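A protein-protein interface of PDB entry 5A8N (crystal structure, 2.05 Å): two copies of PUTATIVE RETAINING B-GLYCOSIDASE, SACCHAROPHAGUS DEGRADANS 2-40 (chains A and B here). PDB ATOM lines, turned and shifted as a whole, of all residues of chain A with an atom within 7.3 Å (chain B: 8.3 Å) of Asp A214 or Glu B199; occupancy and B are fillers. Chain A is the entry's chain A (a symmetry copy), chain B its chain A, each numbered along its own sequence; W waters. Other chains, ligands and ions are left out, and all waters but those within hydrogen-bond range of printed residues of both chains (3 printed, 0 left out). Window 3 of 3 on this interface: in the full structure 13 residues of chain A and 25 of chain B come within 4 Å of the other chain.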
ATOM      1  N   ARG A 165       1.526 -13.190 -18.987  1.00  0.00           N
ATOM      2  CA  ARG A 165       0.480 -13.991 -19.623  1.00  0.00           C
ATOM      3  C   ARG A 165       0.558 -13.883 -21.140  1.00  0.00           C
ATOM      4  O   ARG A 165       0.478 -14.877 -21.855  1.00  0.00           O
ATOM      5  CB  ARG A 165      -0.892 -13.512 -19.176  1.00  0.00           C
ATOM      6  CG  ARG A 165      -1.244 -13.825 -17.728  1.00  0.00           C
ATOM      7  CD  ARG A 165      -2.703 -13.456 -17.478  1.00  0.00           C
ATOM      8  NE  ARG A 165      -3.102 -13.599 -16.094  1.00  0.00           N
ATOM      9  CZ  ARG A 165      -3.451 -14.738 -15.525  1.00  0.00           C
ATOM     10  NH1 ARG A 165      -3.410 -15.860 -16.215  1.00  0.00           N
ATOM     11  NH2 ARG A 165      -3.828 -14.756 -14.254  1.00  0.00           N
ATOM     12  N   THR A 207      -1.127 -20.488  -7.161  1.00  0.00           N
ATOM     13  CA  THR A 207      -2.338 -20.155  -7.916  1.00  0.00           C
ATOM     14  C   THR A 207      -1.998 -19.463  -9.225  1.00  0.00           C
ATOM     15  O   THR A 207      -2.608 -19.720 -10.272  1.00  0.00           O
ATOM     16  CB  THR A 207      -3.265 -19.273  -7.049  1.00  0.00           C
ATOM     17  OG1 THR A 207      -3.661 -20.044  -5.917  1.00  0.00           O
ATOM     18  CG2 THR A 207      -4.514 -18.865  -7.787  1.00  0.00           C
ATOM     19  N   LEU A 208      -1.014 -18.579  -9.178  1.00  0.00           N
ATOM     20  CA  LEU A 208      -0.612 -17.881 -10.397  1.00  0.00           C
ATOM     21  C   LEU A 208       0.009 -18.843 -11.408  1.00  0.00           C
ATOM     22  O   LEU A 208      -0.338 -18.816 -12.598  1.00  0.00           O
ATOM     23  CB  LEU A 208       0.327 -16.723 -10.046  1.00  0.00           C
ATOM     24  CG  LEU A 208       0.732 -15.759 -11.162  1.00  0.00           C
ATOM     25  CD1 LEU A 208      -0.452 -15.275 -11.987  1.00  0.00           C
ATOM     26  CD2 LEU A 208       1.469 -14.586 -10.556  1.00  0.00           C
ATOM     27  N   ASN A 209       0.910 -19.713 -10.958  1.00  0.00           N
ATOM     28  CA  ASN A 209       1.450 -20.746 -11.862  1.00  0.00           C
ATOM     29  C   ASN A 209       0.372 -21.625 -12.452  1.00  0.00           C
ATOM     30  O   ASN A 209       0.393 -21.947 -13.639  1.00  0.00           O
ATOM     31  CB  ASN A 209       2.508 -21.605 -11.167  1.00  0.00           C
ATOM     32  CG  ASN A 209       3.857 -20.906 -11.089  1.00  0.00           C
ATOM     33  OD1 ASN A 209       4.746 -21.115 -11.917  1.00  0.00           O
ATOM     34  ND2 ASN A 209       3.996 -20.040 -10.122  1.00  0.00           N
ATOM     35  N   GLU A 210      -0.583 -22.021 -11.613  1.00  0.00           N
ATOM     36  CA  GLU A 210      -1.712 -22.807 -12.103  1.00  0.00           C
ATOM     37  C   GLU A 210      -2.492 -22.054 -13.172  1.00  0.00           C
ATOM     38  O   GLU A 210      -2.922 -22.650 -14.153  1.00  0.00           O
ATOM     39  CB  GLU A 210      -2.621 -23.241 -10.949  1.00  0.00           C
ATOM     40  CG  GLU A 210      -2.013 -24.364 -10.116  1.00  0.00           C
ATOM     41  CD  GLU A 210      -2.712 -24.612  -8.796  1.00  0.00           C
ATOM     42  OE1 GLU A 210      -3.660 -23.862  -8.451  1.00  0.00           O
ATOM     43  OE2 GLU A 210      -2.289 -25.549  -8.064  1.00  0.00           O
ATOM     44  N   SER A 211      -2.677 -20.748 -12.985  1.00  0.00           N
ATOM     45  CA  SER A 211      -3.362 -19.916 -13.980  1.00  0.00           C
ATOM     46  C   SER A 211      -2.594 -19.929 -15.326  1.00  0.00           C
ATOM     47  O   SER A 211      -3.191 -20.059 -16.404  1.00  0.00           O
ATOM     48  CB  SER A 211      -3.490 -18.479 -13.449  1.00  0.00           C
ATOM     49  OG  SER A 211      -4.255 -17.677 -14.334  1.00  0.00           O
ATOM     50  N   LEU A 212      -1.273 -19.794 -15.258  1.00  0.00           N
ATOM     51  CA  LEU A 212      -0.422 -19.791 -16.464  1.00  0.00           C
ATOM     52  C   LEU A 212      -0.475 -21.136 -17.160  1.00  0.00           C
ATOM     53  O   LEU A 212      -0.619 -21.199 -18.387  1.00  0.00           O
ATOM     54  CB  LEU A 212       1.026 -19.434 -16.144  1.00  0.00           C
ATOM     55  CG  LEU A 212       1.256 -17.965 -15.722  1.00  0.00           C
ATOM     56  CD1 LEU A 212       2.677 -17.742 -15.249  1.00  0.00           C
ATOM     57  CD2 LEU A 212       0.883 -17.004 -16.852  1.00  0.00           C
ATOM     58  N   ILE A 213      -0.384 -22.201 -16.363  1.00  0.00           N
ATOM     59  CA  ILE A 213      -0.438 -23.543 -16.891  1.00  0.00           C
ATOM     60  C   ILE A 213      -1.752 -23.770 -17.623  1.00  0.00           C
ATOM     61  O   ILE A 213      -1.764 -24.368 -18.698  1.00  0.00           O
ATOM     62  CB  ILE A 213      -0.206 -24.603 -15.795  1.00  0.00           C
ATOM     63  CG1 ILE A 213       1.231 -24.568 -15.344  1.00  0.00           C
ATOM     64  CG2 ILE A 213      -0.546 -26.014 -16.285  1.00  0.00           C
ATOM     65  CD1 ILE A 213       1.440 -25.128 -13.952  1.00  0.00           C
ATOM     66  N   ASP A 214      -2.848 -23.287 -17.058  1.00  0.00           N
ATOM     67  CA  ASP A 214      -4.143 -23.496 -17.679  1.00  0.00           C
ATOM     68  C   ASP A 214      -4.220 -22.792 -19.041  1.00  0.00           C
ATOM     69  O   ASP A 214      -4.780 -23.340 -19.991  1.00  0.00           O
ATOM     70  CB  ASP A 214      -5.273 -23.010 -16.795  1.00  0.00           C
ATOM     71  CG  ASP A 214      -5.522 -23.924 -15.603  1.00  0.00           C
ATOM     72  OD1 ASP A 214      -5.080 -25.089 -15.594  1.00  0.00           O
ATOM     73  OD2 ASP A 214      -6.145 -23.447 -14.642  1.00  0.00           O
ATOM     74  N   MET A 215      -3.663 -21.589 -19.138  1.00  0.00           N
ATOM     75  CA  MET A 215      -3.608 -20.877 -20.440  1.00  0.00           C
ATOM     76  C   MET A 215      -2.796 -21.671 -21.447  1.00  0.00           C
ATOM     77  O   MET A 215      -3.146 -21.755 -22.637  1.00  0.00           O
ATOM     78  CB  MET A 215      -2.943 -19.502 -20.327  1.00  0.00           C
ATOM     79  CG  MET A 215      -3.741 -18.426 -19.649  1.00  0.00           C
ATOM     80  SD  MET A 215      -2.753 -16.899 -19.595  1.00  0.00           S
ATOM     81  CE  MET A 215      -3.022 -16.303 -21.259  1.00  0.00           C
ATOM     82  N   ILE A 216      -1.672 -22.191 -20.981  1.00  0.00           N
ATOM     83  CA  ILE A 216      -0.760 -22.922 -21.861  1.00  0.00           C
ATOM     84  C   ILE A 216      -1.430 -24.194 -22.366  1.00  0.00           C
ATOM     85  O   ILE A 216      -1.433 -24.451 -23.562  1.00  0.00           O
ATOM     86  CB  ILE A 216       0.557 -23.238 -21.138  1.00  0.00           C
ATOM     87  CG1 ILE A 216       1.337 -21.939 -20.900  1.00  0.00           C
ATOM     88  CG2 ILE A 216       1.398 -24.221 -21.927  1.00  0.00           C
ATOM     89  CD1 ILE A 216       2.421 -22.060 -19.849  1.00  0.00           C
ATOM     90  N   TYR A 217      -2.022 -24.968 -21.450  1.00  0.00           N
ATOM     91  CA  TYR A 217      -2.637 -26.254 -21.803  1.00  0.00           C
ATOM     92  C   TYR A 217      -3.884 -26.087 -22.663  1.00  0.00           C
ATOM     93  O   TYR A 217      -4.207 -26.982 -23.430  1.00  0.00           O
ATOM     94  CB  TYR A 217      -2.972 -27.104 -20.554  1.00  0.00           C
ATOM     95  CG  TYR A 217      -1.792 -27.820 -19.868  1.00  0.00           C
ATOM     96  CD1 TYR A 217      -0.556 -27.965 -20.492  1.00  0.00           C
ATOM     97  CD2 TYR A 217      -1.951 -28.407 -18.605  1.00  0.00           C
ATOM     98  CE1 TYR A 217       0.485 -28.636 -19.875  1.00  0.00           C
ATOM     99  CE2 TYR A 217      -0.913 -29.088 -17.990  1.00  0.00           C
ATOM    100  CZ  TYR A 217       0.300 -29.202 -18.635  1.00  0.00           C
ATOM    101  OH  TYR A 217       1.338 -29.871 -18.019  1.00  0.00           O
ATOM    102  N   ALA A 218      -4.571 -24.949 -22.538  1.00  0.00           N
ATOM    103  CA  ALA A 218      -5.721 -24.653 -23.394  1.00  0.00           C
ATOM    104  C   ALA A 218      -5.310 -24.473 -24.862  1.00  0.00           C
ATOM    105  O   ALA A 218      -6.149 -24.591 -25.749  1.00  0.00           O
ATOM    106  CB  ALA A 218      -6.458 -23.410 -22.899  1.00  0.00           C
ATOM    107  N   SER A 219      -4.027 -24.188 -25.087  1.00  0.00           N
ATOM    108  CA  SER A 219      -3.449 -23.914 -26.414  1.00  0.00           C
ATOM    109  C   SER A 219      -2.554 -25.070 -26.930  1.00  0.00           C
ATOM    110  O   SER A 219      -2.510 -25.312 -28.129  1.00  0.00           O
ATOM    111  CB  SER A 219      -2.630 -22.605 -26.316  1.00  0.00           C
ATOM    112  OG  SER A 219      -1.988 -22.223 -27.534  1.00  0.00           O
ATOM    113  N   ASP A 220      -1.845 -25.768 -26.030  1.00  0.00           N
ATOM    114  CA  ASP A 220      -0.957 -26.895 -26.390  1.00  0.00           C
ATOM    115  C   ASP A 220      -0.731 -27.811 -25.199  1.00  0.00           C
ATOM    116  O   ASP A 220      -0.046 -27.428 -24.242  1.00  0.00           O
ATOM    117  CB  ASP A 220       0.402 -26.374 -26.871  1.00  0.00           C
ATOM    118  CG  ASP A 220       1.303 -27.474 -27.487  1.00  0.00           C
ATOM    119  OD1 ASP A 220       1.022 -28.686 -27.344  1.00  0.00           O
ATOM    120  OD2 ASP A 220       2.326 -27.112 -28.105  1.00  0.00           O
ATOM    121  N   PRO A 225       5.376 -27.508 -18.779  1.00  0.00           N
ATOM    122  CA  PRO A 225       5.631 -26.349 -17.923  1.00  0.00           C
ATOM    123  C   PRO A 225       6.623 -26.669 -16.813  1.00  0.00           C
ATOM    124  O   PRO A 225       6.616 -27.770 -16.263  1.00  0.00           O
ATOM    125  CB  PRO A 225       4.251 -26.015 -17.320  1.00  0.00           C
ATOM    126  CG  PRO A 225       3.271 -26.837 -18.084  1.00  0.00           C
ATOM    127  CD  PRO A 225       4.031 -28.048 -18.555  1.00  0.00           C
ATOM    128  N   GLU A 245      -1.284 -28.167  -8.588  1.00  0.00           N
ATOM    129  CA  GLU A 245      -2.306 -29.207  -8.818  1.00  0.00           C
ATOM    130  C   GLU A 245      -2.593 -29.414 -10.308  1.00  0.00           C
ATOM    131  O   GLU A 245      -3.723 -29.345 -10.752  1.00  0.00           O
ATOM    132  CB  GLU A 245      -3.566 -28.862  -8.022  1.00  0.00           C
ATOM    133  CG  GLU A 245      -3.301 -28.891  -6.526  1.00  0.00           C
ATOM    134  CD  GLU A 245      -4.515 -28.565  -5.694  1.00  0.00           C
ATOM    135  OE1 GLU A 245      -5.474 -29.346  -5.711  1.00  0.00           O
ATOM    136  OE2 GLU A 245      -4.504 -27.535  -5.003  1.00  0.00           O
ATOM    137  N   ARG A 246      -1.539 -29.662 -11.081  1.00  0.00           N
ATOM    138  CA  ARG A 246      -1.656 -29.906 -12.506  1.00  0.00           C
ATOM    139  C   ARG A 246      -0.691 -31.023 -12.844  1.00  0.00           C
ATOM    140  O   ARG A 246       0.393 -31.116 -12.252  1.00  0.00           O
ATOM    141  CB  ARG A 246      -1.288 -28.648 -13.298  1.00  0.00           C
ATOM    142  CG  ARG A 246      -2.166 -27.417 -13.019  1.00  0.00           C
ATOM    143  CD  ARG A 246      -3.578 -27.577 -13.572  1.00  0.00           C
ATOM    144  NE  ARG A 246      -4.394 -26.375 -13.379  1.00  0.00           N
ATOM    145  CZ  ARG A 246      -5.044 -26.044 -12.264  1.00  0.00           C
ATOM    146  NH1 ARG A 246      -4.958 -26.777 -11.168  1.00  0.00           N
ATOM    147  NH2 ARG A 246      -5.764 -24.940 -12.242  1.00  0.00           N
ATOM    148  N   TYR B 146     -10.845 -11.180 -22.492  1.00  0.00           N
ATOM    149  CA  TYR B 146     -11.130 -11.424 -21.098  1.00  0.00           C
ATOM    150  C   TYR B 146     -10.498 -10.371 -20.209  1.00  0.00           C
ATOM    151  O   TYR B 146      -9.311 -10.446 -19.871  1.00  0.00           O
ATOM    152  CB  TYR B 146     -10.659 -12.818 -20.688  1.00  0.00           C
ATOM    153  CG  TYR B 146     -11.363 -13.323 -19.454  1.00  0.00           C
ATOM    154  CD1 TYR B 146     -12.765 -13.403 -19.407  1.00  0.00           C
ATOM    155  CD2 TYR B 146     -10.652 -13.735 -18.332  1.00  0.00           C
ATOM    156  CE1 TYR B 146     -13.416 -13.864 -18.274  1.00  0.00           C
ATOM    157  CE2 TYR B 146     -11.311 -14.210 -17.193  1.00  0.00           C
ATOM    158  CZ  TYR B 146     -12.687 -14.280 -17.184  1.00  0.00           C
ATOM    159  OH  TYR B 146     -13.358 -14.736 -16.071  1.00  0.00           O
ATOM    160  N   PRO B 148     -10.745  -9.639 -16.999  1.00  0.00           N
ATOM    161  CA  PRO B 148     -10.118  -9.985 -15.730  1.00  0.00           C
ATOM    162  C   PRO B 148      -8.652 -10.406 -15.829  1.00  0.00           C
ATOM    163  O   PRO B 148      -7.913 -10.167 -14.899  1.00  0.00           O
ATOM    164  CB  PRO B 148     -11.010 -11.138 -15.198  1.00  0.00           C
ATOM    165  CG  PRO B 148     -12.342 -10.842 -15.780  1.00  0.00           C
ATOM    166  CD  PRO B 148     -12.028 -10.358 -17.171  1.00  0.00           C
ATOM    167  N   THR B 149      -8.218 -11.019 -16.934  1.00  0.00           N
ATOM    168  CA  THR B 149      -6.806 -11.337 -17.114  1.00  0.00           C
ATOM    169  C   THR B 149      -6.099 -10.358 -18.049  1.00  0.00           C
ATOM    170  O   THR B 149      -4.898 -10.473 -18.292  1.00  0.00           O
ATOM    171  CB  THR B 149      -6.608 -12.751 -17.708  1.00  0.00           C
ATOM    172  OG1 THR B 149      -7.369 -12.856 -18.909  1.00  0.00           O
ATOM    173  CG2 THR B 149      -7.043 -13.840 -16.723  1.00  0.00           C
ATOM    174  N   THR B 191     -14.858 -13.075 -24.021  1.00  0.00           N
ATOM    175  CA  THR B 191     -14.514 -14.429 -24.469  1.00  0.00           C
ATOM    176  C   THR B 191     -13.149 -14.808 -23.912  1.00  0.00           C
ATOM    177  O   THR B 191     -12.283 -13.951 -23.751  1.00  0.00           O
ATOM    178  CB  THR B 191     -14.515 -14.578 -26.020  1.00  0.00           C
ATOM    179  OG1 THR B 191     -14.100 -15.911 -26.373  1.00  0.00           O
ATOM    180  CG2 THR B 191     -13.589 -13.558 -26.696  1.00  0.00           C
ATOM    181  N   THR B 192     -12.947 -16.079 -23.588  1.00  0.00           N
ATOM    182  CA  THR B 192     -11.591 -16.545 -23.264  1.00  0.00           C
ATOM    183  C   THR B 192     -10.935 -17.326 -24.412  1.00  0.00           C
ATOM    184  O   THR B 192      -9.844 -17.897 -24.239  1.00  0.00           O
ATOM    185  CB  THR B 192     -11.581 -17.440 -22.030  1.00  0.00           C
ATOM    186  OG1 THR B 192     -12.412 -18.595 -22.289  1.00  0.00           O
ATOM    187  CG2 THR B 192     -12.062 -16.670 -20.797  1.00  0.00           C
ATOM    188  N   GLY B 194     -11.674 -20.304 -25.892  1.00  0.00           N
ATOM    189  CA  GLY B 194     -11.393 -21.671 -25.477  1.00  0.00           C
ATOM    190  C   GLY B 194     -10.504 -21.739 -24.239  1.00  0.00           C
ATOM    191  O   GLY B 194      -9.754 -22.700 -24.054  1.00  0.00           O
ATOM    192  N   ASN B 195     -10.590 -20.718 -23.388  1.00  0.00           N
ATOM    193  CA  ASN B 195      -9.753 -20.606 -22.189  1.00  0.00           C
ATOM    194  C   ASN B 195      -8.248 -20.412 -22.448  1.00  0.00           C
ATOM    195  O   ASN B 195      -7.417 -20.582 -21.549  1.00  0.00           O
ATOM    196  CB  ASN B 195     -10.037 -21.760 -21.202  1.00  0.00           C
ATOM    197  CG  ASN B 195     -11.308 -21.537 -20.405  1.00  0.00           C
ATOM    198  OD1 ASN B 195     -11.946 -20.487 -20.487  1.00  0.00           O
ATOM    199  ND2 ASN B 195     -11.657 -22.508 -19.599  1.00  0.00           N
ATOM    200  N   THR B 196      -7.905 -19.986 -23.661  1.00  0.00           N
ATOM    201  CA  THR B 196      -6.530 -19.623 -23.978  1.00  0.00           C
ATOM    202  C   THR B 196      -6.200 -18.242 -23.415  1.00  0.00           C
ATOM    203  O   THR B 196      -5.028 -17.894 -23.278  1.00  0.00           O
ATOM    204  CB  THR B 196      -6.256 -19.617 -25.500  1.00  0.00           C
ATOM    205  OG1 THR B 196      -7.173 -18.745 -26.161  1.00  0.00           O
ATOM    206  CG2 THR B 196      -6.405 -20.997 -26.099  1.00  0.00           C
ATOM    207  N   LEU B 197      -7.219 -17.440 -23.106  1.00  0.00           N
ATOM    208  CA  LEU B 197      -7.003 -16.071 -22.597  1.00  0.00           C
ATOM    209  C   LEU B 197      -7.070 -16.000 -21.081  1.00  0.00           C
ATOM    210  O   LEU B 197      -6.692 -14.985 -20.496  1.00  0.00           O
ATOM    211  CB  LEU B 197      -8.024 -15.111 -23.186  1.00  0.00           C
ATOM    212  CG  LEU B 197      -8.016 -14.948 -24.707  1.00  0.00           C
ATOM    213  CD1 LEU B 197      -8.949 -13.820 -25.086  1.00  0.00           C
ATOM    214  CD2 LEU B 197      -6.613 -14.687 -25.222  1.00  0.00           C
ATOM    215  N   GLY B 198      -7.521 -17.091 -20.461  1.00  0.00           N
ATOM    216  CA  GLY B 198      -7.784 -17.159 -19.013  1.00  0.00           C
ATOM    217  C   GLY B 198      -8.877 -18.188 -18.778  1.00  0.00           C
ATOM    218  O   GLY B 198      -9.383 -18.757 -19.738  1.00  0.00           O
ATOM    219  N   GLU B 199      -9.234 -18.438 -17.518  1.00  0.00           N
ATOM    220  CA  GLU B 199     -10.310 -19.395 -17.188  1.00  0.00           C
ATOM    221  C   GLU B 199     -11.576 -18.590 -17.032  1.00  0.00           C
ATOM    222  O   GLU B 199     -11.665 -17.774 -16.122  1.00  0.00           O
ATOM    223  CB  GLU B 199     -10.017 -20.149 -15.876  1.00  0.00           C
ATOM    224  CG  GLU B 199      -8.894 -21.178 -15.957  1.00  0.00           C
ATOM    225  CD  GLU B 199      -9.316 -22.439 -16.703  1.00  0.00           C
ATOM    226  OE1 GLU B 199     -10.252 -23.109 -16.225  1.00  0.00           O
ATOM    227  OE2 GLU B 199      -8.735 -22.744 -17.775  1.00  0.00           O
ATOM    228  N   ARG B 200     -12.547 -18.773 -17.926  1.00  0.00           N
ATOM    229  CA  ARG B 200     -13.784 -18.007 -17.844  1.00  0.00           C
ATOM    230  C   ARG B 200     -14.409 -18.341 -16.519  1.00  0.00           C
ATOM    231  O   ARG B 200     -14.413 -19.510 -16.108  1.00  0.00           O
ATOM    232  CB  ARG B 200     -14.738 -18.320 -18.997  1.00  0.00           C
ATOM    233  CG  ARG B 200     -15.361 -19.720 -18.971  1.00  0.00           C
ATOM    234  CD  ARG B 200     -16.245 -19.926 -20.193  1.00  0.00           C
ATOM    235  NE  ARG B 200     -15.473 -20.057 -21.430  1.00  0.00           N
ATOM    236  CZ  ARG B 200     -14.903 -21.176 -21.841  1.00  0.00           C
ATOM    237  NH1 ARG B 200     -15.011 -22.297 -21.125  1.00  0.00           N
ATOM    238  NH2 ARG B 200     -14.231 -21.188 -22.977  1.00  0.00           N
ATOM    239  N   ASN B 201     -14.861 -17.310 -15.825  1.00  0.00           N
ATOM    240  CA  ASN B 201     -15.448 -17.459 -14.496  1.00  0.00           C
ATOM    241  C   ASN B 201     -16.539 -16.428 -14.349  1.00  0.00           C
ATOM    242  O   ASN B 201     -16.251 -15.238 -14.286  1.00  0.00           O
ATOM    243  CB  ASN B 201     -14.385 -17.248 -13.423  1.00  0.00           C
ATOM    244  CG  ASN B 201     -14.918 -17.500 -12.026  1.00  0.00           C
ATOM    245  OD1 ASN B 201     -15.474 -16.620 -11.384  1.00  0.00           O
ATOM    246  ND2 ASN B 201     -14.754 -18.718 -11.557  1.00  0.00           N
ATOM    247  N   TRP B 202     -17.794 -16.876 -14.310  1.00  0.00           N
ATOM    248  CA  TRP B 202     -18.916 -15.944 -14.283  1.00  0.00           C
ATOM    249  C   TRP B 202     -18.863 -15.042 -13.054  1.00  0.00           C
ATOM    250  O   TRP B 202     -19.047 -13.836 -13.178  1.00  0.00           O
ATOM    251  CB  TRP B 202     -20.285 -16.664 -14.373  1.00  0.00           C
ATOM    252  CG  TRP B 202     -21.382 -15.675 -14.341  1.00  0.00           C
ATOM    253  CD1 TRP B 202     -22.215 -15.412 -13.293  1.00  0.00           C
ATOM    254  CD2 TRP B 202     -21.707 -14.721 -15.359  1.00  0.00           C
ATOM    255  NE1 TRP B 202     -23.063 -14.381 -13.609  1.00  0.00           N
ATOM    256  CE2 TRP B 202     -22.776 -13.939 -14.873  1.00  0.00           C
ATOM    257  CE3 TRP B 202     -21.234 -14.481 -16.651  1.00  0.00           C
ATOM    258  CZ2 TRP B 202     -23.374 -12.925 -15.633  1.00  0.00           C
ATOM    259  CZ3 TRP B 202     -21.842 -13.464 -17.413  1.00  0.00           C
ATOM    260  CH2 TRP B 202     -22.891 -12.706 -16.897  1.00  0.00           C
ATOM    261  N   GLU B 204     -16.464 -13.869 -11.255  1.00  0.00           N
ATOM    262  CA  GLU B 204     -15.444 -12.835 -11.397  1.00  0.00           C
ATOM    263  C   GLU B 204     -15.886 -11.753 -12.397  1.00  0.00           C
ATOM    264  O   GLU B 204     -15.715 -10.550 -12.158  1.00  0.00           O
ATOM    265  CB  GLU B 204     -14.132 -13.535 -11.796  1.00  0.00           C
ATOM    266  CG  GLU B 204     -13.183 -12.814 -12.697  1.00  0.00           C
ATOM    267  CD  GLU B 204     -11.925 -13.650 -12.940  1.00  0.00           C
ATOM    268  OE1 GLU B 204     -11.910 -14.513 -13.853  1.00  0.00           O
ATOM    269  OE2 GLU B 204     -10.955 -13.448 -12.187  1.00  0.00           O
ATOM    270  N   TRP B 205     -16.482 -12.184 -13.500  1.00  0.00           N
ATOM    271  CA  TRP B 205     -16.956 -11.257 -14.534  1.00  0.00           C
ATOM    272  C   TRP B 205     -18.144 -10.427 -14.024  1.00  0.00           C
ATOM    273  O   TRP B 205     -18.174  -9.212 -14.170  1.00  0.00           O
ATOM    274  CB  TRP B 205     -17.304 -12.023 -15.813  1.00  0.00           C
ATOM    275  CG  TRP B 205     -17.770 -11.174 -16.949  1.00  0.00           C
ATOM    276  CD1 TRP B 205     -18.902 -11.330 -17.648  1.00  0.00           C
ATOM    277  CD2 TRP B 205     -17.093 -10.050 -17.521  1.00  0.00           C
ATOM    278  NE1 TRP B 205     -18.979 -10.392 -18.644  1.00  0.00           N
ATOM    279  CE2 TRP B 205     -17.887  -9.579 -18.572  1.00  0.00           C
ATOM    280  CE3 TRP B 205     -15.908  -9.386 -17.228  1.00  0.00           C
ATOM    281  CZ2 TRP B 205     -17.541  -8.462 -19.336  1.00  0.00           C
ATOM    282  CZ3 TRP B 205     -15.574  -8.257 -17.972  1.00  0.00           C
ATOM    283  CH2 TRP B 205     -16.381  -7.820 -19.015  1.00  0.00           C
ATOM    284  N   PHE B 230     -20.536 -14.604 -21.972  1.00  0.00           N
ATOM    285  CA  PHE B 230     -19.370 -15.225 -22.553  1.00  0.00           C
ATOM    286  C   PHE B 230     -19.644 -15.713 -23.980  1.00  0.00           C
ATOM    287  O   PHE B 230     -20.698 -15.440 -24.553  1.00  0.00           O
ATOM    288  CB  PHE B 230     -18.899 -16.379 -21.648  1.00  0.00           C
ATOM    289  CG  PHE B 230     -18.388 -15.943 -20.288  1.00  0.00           C
ATOM    290  CD1 PHE B 230     -17.733 -14.745 -20.110  1.00  0.00           C
ATOM    291  CD2 PHE B 230     -18.515 -16.780 -19.197  1.00  0.00           C
ATOM    292  CE1 PHE B 230     -17.259 -14.367 -18.869  1.00  0.00           C
ATOM    293  CE2 PHE B 230     -18.019 -16.416 -17.957  1.00  0.00           C
ATOM    294  CZ  PHE B 230     -17.376 -15.212 -17.791  1.00  0.00           C
HETATM  295  O   HOH W   1      -3.231 -10.459 -16.107  1.00  0.00           O
HETATM  296  O   HOH W   2      -8.696 -24.592 -25.497  1.00  0.00           O
HETATM  297  O   HOH W   3      -2.904 -19.463 -24.197  1.00  0.00           O
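The backbone carbonyl oxygen of Thr B192 lies within hydrogen-bond range of the backbone NH of Leu B197, at 2.9 Å.
NE of Arg A246 is in salt-bridge range of OD1 of Asp A214 (2.7 Å).
O of Tyr B146 is in hydrogen-bond range of OG1 of Thr B149 (3.2 Å).
OD1 of Asn B195 lies within hydrogen-bond range of N of Arg B200.
The guanidinium group (NH1) of Arg A165 lies within hydrogen-bond range of the side-chain hydroxyl (OG) of Ser A211 (2.7 Å).
The side-chain amide oxygen (OD1) of Asn B195 is in hydrogen-bond range of the side-chain hydroxyl (OG1) of Thr B192 (2.7 Å).
Among the printed residues, pairs that only touch across the chains: Met A215 with Thr B196 (3.3 Å), Ala A218 with Asn B195 (3.3 Å), Ala A218 with Gly B194 (3.6 Å), Asp A214 with Glu B199 (3.6 Å), Ala A218 with Thr B196 (3.6 Å), Arg A165 with Thr B149 (3.8 Å), Met A215 with Leu B197 (3.97 Å) and Met A215 with Asn B195 (3.98 Å).
Of the printed residues of chain B, Asp A214 touches Glu B199.
Thr B192 touches none of the printed residues of chain A.
Printed residues of chain A within 4 Å of Gly B194: Ala A218.
Of the printed residues of chain A, Asn B195 touches Met A215 and Ala A218.
Of the printed residues of chain A, Thr B196 touches Met A215 (3.3 Å) and Ala A218 (3.6 Å).
Glu B199 touches just one residue of chain A: Asp A214 (3.6 Å).
Printed residues of chain B that touch a printed residue of chain A: Thr B149, Gly B194, Asn B195, Thr B196, Leu B197 and Glu B199.
Of the 18 printed residues of chain A, 4 touch a printed residue of chain B.
Printed residues of chain A that touch a printed residue of chain B: Arg A165, Asp A214, Met A215 and Ala A218.
Hydrophobic or aromatic side chains of chain A within 4 Å of the printed part of chain B: Met A215 and Ala A218.
Among the printed residues, no Asp or Glu carboxylate lies within 4 Å of a Lys or Arg side-chain nitrogen of the other chain.
No position is printed for both chains.
Of the 8 pairs that touch across the chains among the printed residues, none has its exchanged pair printed and touching as well.
Water W2 bridges the backbone carbonyl oxygen of Ala A218 and the backbone carbonyl oxygen of Gly B194.
Water W1 bridges O of Thr B149 (2.7 Å) and NE of Arg A165 (3.1 Å).
Water W3 bridges O of Met A215 (2.8 Å) and O of Thr B196 (2.8 Å).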
